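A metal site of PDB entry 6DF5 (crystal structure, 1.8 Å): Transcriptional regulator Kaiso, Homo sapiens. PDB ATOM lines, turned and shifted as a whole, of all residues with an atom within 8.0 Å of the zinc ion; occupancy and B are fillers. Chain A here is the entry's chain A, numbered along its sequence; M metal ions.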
ATOM      1  N   PRO A  53     -23.482 -17.142 -20.100  1.00  0.00           N
ATOM      2  CA  PRO A  53     -24.531 -16.197 -20.473  1.00  0.00           C
ATOM      3  C   PRO A  53     -24.615 -15.991 -21.980  1.00  0.00           C
ATOM      4  O   PRO A  53     -23.565 -15.905 -22.621  1.00  0.00           O
ATOM      5  CB  PRO A  53     -24.100 -14.917 -19.779  1.00  0.00           C
ATOM      6  CG  PRO A  53     -22.594 -15.001 -19.791  1.00  0.00           C
ATOM      7  CD  PRO A  53     -22.246 -16.466 -19.672  1.00  0.00           C
ATOM      8  N   CYS A  54     -25.822 -15.958 -22.543  1.00  0.00           N
ATOM      9  CA  CYS A  54     -26.031 -15.585 -23.946  1.00  0.00           C
ATOM     10  C   CYS A  54     -25.433 -14.222 -24.254  1.00  0.00           C
ATOM     11  O   CYS A  54     -25.667 -13.265 -23.534  1.00  0.00           O
ATOM     12  CB  CYS A  54     -27.529 -15.562 -24.270  1.00  0.00           C
ATOM     13  SG  CYS A  54     -27.930 -15.143 -26.043  1.00  0.00           S
ATOM     14  N   ARG A  55     -24.674 -14.118 -25.339  1.00  0.00           N
ATOM     15  CA  ARG A  55     -24.063 -12.824 -25.647  1.00  0.00           C
ATOM     16  C   ARG A  55     -25.066 -11.839 -26.274  1.00  0.00           C
ATOM     17  O   ARG A  55     -24.733 -10.685 -26.513  1.00  0.00           O
ATOM     18  CB  ARG A  55     -22.844 -13.014 -26.578  1.00  0.00           C
ATOM     19  CG  ARG A  55     -23.162 -12.885 -28.083  1.00  0.00           C
ATOM     20  CD  ARG A  55     -21.963 -13.172 -29.009  1.00  0.00           C
ATOM     21  NE  ARG A  55     -21.572 -14.587 -29.007  1.00  0.00           N
ATOM     22  CZ  ARG A  55     -20.728 -15.138 -29.873  1.00  0.00           C
ATOM     23  NH1 ARG A  55     -20.180 -14.392 -30.821  1.00  0.00           N
ATOM     24  NH2 ARG A  55     -20.428 -16.429 -29.780  1.00  0.00           N
ATOM     25  N   TYR A  56     -26.297 -12.283 -26.547  1.00  0.00           N
ATOM     26  CA  TYR A  56     -27.294 -11.416 -27.183  1.00  0.00           C
ATOM     27  C   TYR A  56     -28.486 -11.079 -26.301  1.00  0.00           C
ATOM     28  O   TYR A  56     -29.186 -10.106 -26.529  1.00  0.00           O
ATOM     29  CB  TYR A  56     -27.825 -12.048 -28.471  1.00  0.00           C
ATOM     30  CG  TYR A  56     -26.773 -12.378 -29.493  1.00  0.00           C
ATOM     31  CD1 TYR A  56     -26.280 -13.675 -29.609  1.00  0.00           C
ATOM     32  CD2 TYR A  56     -26.286 -11.404 -30.353  1.00  0.00           C
ATOM     33  CE1 TYR A  56     -25.313 -13.987 -30.555  1.00  0.00           C
ATOM     34  CE2 TYR A  56     -25.319 -11.716 -31.299  1.00  0.00           C
ATOM     35  CZ  TYR A  56     -24.841 -12.997 -31.394  1.00  0.00           C
ATOM     36  OH  TYR A  56     -23.881 -13.302 -32.325  1.00  0.00           O
ATOM     37  N   CYS A  57     -28.770 -11.923 -25.316  1.00  0.00           N
ATOM     38  CA  CYS A  57     -29.859 -11.629 -24.404  1.00  0.00           C
ATOM     39  C   CYS A  57     -29.460 -12.005 -22.976  1.00  0.00           C
ATOM     40  O   CYS A  57     -28.295 -12.275 -22.698  1.00  0.00           O
ATOM     41  CB  CYS A  57     -31.150 -12.349 -24.832  1.00  0.00           C
ATOM     42  SG  CYS A  57     -31.198 -14.092 -24.388  1.00  0.00           S
ATOM     43  N   GLU A  58     -30.444 -12.029 -22.087  1.00  0.00           N
ATOM     44  CA  GLU A  58     -30.197 -12.116 -20.652  1.00  0.00           C
ATOM     45  C   GLU A  58     -30.078 -13.551 -20.153  1.00  0.00           C
ATOM     46  O   GLU A  58     -29.700 -13.783 -19.011  1.00  0.00           O
ATOM     47  CB  GLU A  58     -31.321 -11.389 -19.896  1.00  0.00           C
ATOM     48  CG  GLU A  58     -32.676 -12.137 -19.908  1.00  0.00           C
ATOM     49  CD  GLU A  58     -33.384 -12.092 -21.269  1.00  0.00           C
ATOM     50  OE1 GLU A  58     -34.184 -13.013 -21.540  1.00  0.00           O
ATOM     51  OE2 GLU A  58     -33.141 -11.148 -22.049  1.00  0.00           O
ATOM     52  N   LYS A  59     -30.388 -14.516 -21.026  1.00  0.00           N
ATOM     53  CA  LYS A  59     -30.396 -15.923 -20.617  1.00  0.00           C
ATOM     54  C   LYS A  59     -29.009 -16.451 -20.266  1.00  0.00           C
ATOM     55  O   LYS A  59     -28.002 -16.033 -20.843  1.00  0.00           O
ATOM     56  CB  LYS A  59     -31.025 -16.784 -21.704  1.00  0.00           C
ATOM     57  CG  LYS A  59     -32.529 -16.874 -21.591  1.00  0.00           C
ATOM     58  CD  LYS A  59     -33.134 -17.596 -22.787  1.00  0.00           C
ATOM     59  CE  LYS A  59     -34.632 -17.410 -22.841  1.00  0.00           C
ATOM     60  NZ  LYS A  59     -35.156 -17.622 -24.221  1.00  0.00           N
ATOM     61  N   VAL A  60     -28.968 -17.368 -19.308  1.00  0.00           N
ATOM     62  CA  VAL A  60     -27.725 -17.941 -18.834  1.00  0.00           C
ATOM     63  C   VAL A  60     -27.842 -19.455 -18.808  1.00  0.00           C
ATOM     64  O   VAL A  60     -28.866 -19.997 -18.404  1.00  0.00           O
ATOM     65  CB  VAL A  60     -27.367 -17.424 -17.426  1.00  0.00           C
ATOM     66  CG1 VAL A  60     -26.056 -18.017 -16.960  1.00  0.00           C
ATOM     67  CG2 VAL A  60     -27.298 -15.905 -17.442  1.00  0.00           C
ATOM     68  N   PHE A  61     -26.786 -20.153 -19.253  1.00  0.00           N
ATOM     69  CA  PHE A  61     -26.812 -21.605 -19.369  1.00  0.00           C
ATOM     70  C   PHE A  61     -25.771 -22.302 -18.499  1.00  0.00           C
ATOM     71  O   PHE A  61     -24.723 -21.733 -18.233  1.00  0.00           O
ATOM     72  CB  PHE A  61     -26.615 -22.007 -20.833  1.00  0.00           C
ATOM     73  CG  PHE A  61     -27.686 -21.495 -21.746  1.00  0.00           C
ATOM     74  CD1 PHE A  61     -28.778 -22.289 -22.060  1.00  0.00           C
ATOM     75  CD2 PHE A  61     -27.604 -20.213 -22.287  1.00  0.00           C
ATOM     76  CE1 PHE A  61     -29.768 -21.820 -22.905  1.00  0.00           C
ATOM     77  CE2 PHE A  61     -28.591 -19.739 -23.119  1.00  0.00           C
ATOM     78  CZ  PHE A  61     -29.682 -20.537 -23.425  1.00  0.00           C
ATOM     79  N   ARG A  67     -25.493 -22.926 -24.517  1.00  0.00           N
ATOM     80  CA  ARG A  67     -25.451 -21.518 -24.865  1.00  0.00           C
ATOM     81  C   ARG A  67     -25.198 -21.335 -26.366  1.00  0.00           C
ATOM     82  O   ARG A  67     -25.821 -20.490 -27.014  1.00  0.00           O
ATOM     83  CB  ARG A  67     -24.381 -20.774 -24.072  1.00  0.00           C
ATOM     84  CG  ARG A  67     -24.211 -19.333 -24.613  1.00  0.00           C
ATOM     85  CD  ARG A  67     -23.152 -18.587 -23.873  1.00  0.00           C
ATOM     86  NE  ARG A  67     -21.847 -19.221 -24.030  1.00  0.00           N
ATOM     87  CZ  ARG A  67     -20.748 -18.768 -23.448  1.00  0.00           C
ATOM     88  NH1 ARG A  67     -20.809 -17.682 -22.697  1.00  0.00           N
ATOM     89  NH2 ARG A  67     -19.590 -19.399 -23.625  1.00  0.00           N
ATOM     90  N   HIS A  70     -28.205 -22.047 -28.559  1.00  0.00           N
ATOM     91  CA  HIS A  70     -29.096 -20.926 -28.339  1.00  0.00           C
ATOM     92  C   HIS A  70     -28.672 -19.674 -29.099  1.00  0.00           C
ATOM     93  O   HIS A  70     -29.509 -18.935 -29.629  1.00  0.00           O
ATOM     94  CB  HIS A  70     -29.164 -20.601 -26.851  1.00  0.00           C
ATOM     95  CG  HIS A  70     -29.891 -19.332 -26.558  1.00  0.00           C
ATOM     96  ND1 HIS A  70     -31.269 -19.240 -26.572  1.00  0.00           N
ATOM     97  CD2 HIS A  70     -29.430 -18.097 -26.251  1.00  0.00           C
ATOM     98  CE1 HIS A  70     -31.627 -18.005 -26.262  1.00  0.00           C
ATOM     99  NE2 HIS A  70     -30.533 -17.290 -26.049  1.00  0.00           N
ATOM    100  N   GLU A  71     -27.365 -19.397 -29.122  1.00  0.00           N
ATOM    101  CA  GLU A  71     -26.879 -18.203 -29.797  1.00  0.00           C
ATOM    102  C   GLU A  71     -27.033 -18.342 -31.312  1.00  0.00           C
ATOM    103  O   GLU A  71     -27.200 -17.338 -32.025  1.00  0.00           O
ATOM    104  CB  GLU A  71     -25.421 -17.930 -29.425  1.00  0.00           C
ATOM    105  CG  GLU A  71     -25.280 -17.368 -27.998  1.00  0.00           C
ATOM    106  CD  GLU A  71     -23.853 -17.062 -27.640  1.00  0.00           C
ATOM    107  OE1 GLU A  71     -22.951 -17.710 -28.216  1.00  0.00           O
ATOM    108  OE2 GLU A  71     -23.618 -16.168 -26.798  1.00  0.00           O
ATOM    109  N   ILE A  72     -26.997 -19.574 -31.803  1.00  0.00           N
ATOM    110  CA  ILE A  72     -27.182 -19.777 -33.232  1.00  0.00           C
ATOM    111  C   ILE A  72     -28.631 -19.432 -33.587  1.00  0.00           C
ATOM    112  O   ILE A  72     -28.892 -18.921 -34.657  1.00  0.00           O
ATOM    113  CB  ILE A  72     -26.820 -21.211 -33.674  1.00  0.00           C
ATOM    114  CG1 ILE A  72     -25.307 -21.290 -33.862  1.00  0.00           C
ATOM    115  CG2 ILE A  72     -27.465 -21.558 -35.018  1.00  0.00           C
ATOM    116  CD1 ILE A  72     -24.731 -22.679 -33.766  1.00  0.00           C
ATOM    117  N   HIS A  73     -29.557 -19.657 -32.663  1.00  0.00           N
ATOM    118  CA  HIS A  73     -30.933 -19.188 -32.875  1.00  0.00           C
ATOM    119  C   HIS A  73     -31.020 -17.687 -33.096  1.00  0.00           C
ATOM    120  O   HIS A  73     -31.761 -17.217 -33.979  1.00  0.00           O
ATOM    121  CB  HIS A  73     -31.833 -19.545 -31.693  1.00  0.00           C
ATOM    122  CG  HIS A  73     -32.539 -20.851 -31.850  1.00  0.00           C
ATOM    123  ND1 HIS A  73     -33.672 -20.989 -32.620  1.00  0.00           N
ATOM    124  CD2 HIS A  73     -32.281 -22.076 -31.336  1.00  0.00           C
ATOM    125  CE1 HIS A  73     -34.078 -22.254 -32.585  1.00  0.00           C
ATOM    126  NE2 HIS A  73     -33.256 -22.928 -31.804  1.00  0.00           N
ATOM    127  N   HIS A  74     -30.303 -16.917 -32.283  1.00  0.00           N
ATOM    128  CA  HIS A  74     -30.286 -15.472 -32.467  1.00  0.00           C
ATOM    129  C   HIS A  74     -29.842 -15.038 -33.866  1.00  0.00           C
ATOM    130  O   HIS A  74     -30.410 -14.116 -34.433  1.00  0.00           O
ATOM    131  CB  HIS A  74     -29.374 -14.818 -31.436  1.00  0.00           C
ATOM    132  CG  HIS A  74     -30.000 -14.658 -30.091  1.00  0.00           C
ATOM    133  ND1 HIS A  74     -30.904 -13.653 -29.820  1.00  0.00           N
ATOM    134  CD2 HIS A  74     -29.846 -15.356 -28.943  1.00  0.00           C
ATOM    135  CE1 HIS A  74     -31.285 -13.738 -28.553  1.00  0.00           C
ATOM    136  NE2 HIS A  74     -30.663 -14.771 -28.010  1.00  0.00           N
HETATM  137 ZN    ZN M   1     -30.084 -15.238 -26.043  1.00  0.00          ZN
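The zinc ion is bound by a ring nitrogen (NE2) of His 70 (2.1 Å), a ring nitrogen (NE2) of His 74 (2.1 Å), the side-chain sulfur (SG) of Cys 54 (2.2 Å) and the side-chain sulfur (SG) of Cys 57 (2.3 Å).
The zinc ion has four donor atoms within binding distance.
Of the 15 residues printed, 4 come within 4 Å of the zinc ion.
SG of Cys 57 lies close to N of Lys 59, 3.5 Å away.
O of Lys 59 lies within hydrogen-bond range of N of Cys 54 (2.8 Å).
The side-chain sulfur (SG) of Cys 54 lies close to the backbone NH (N) of Tyr 56 (3.3 Å).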
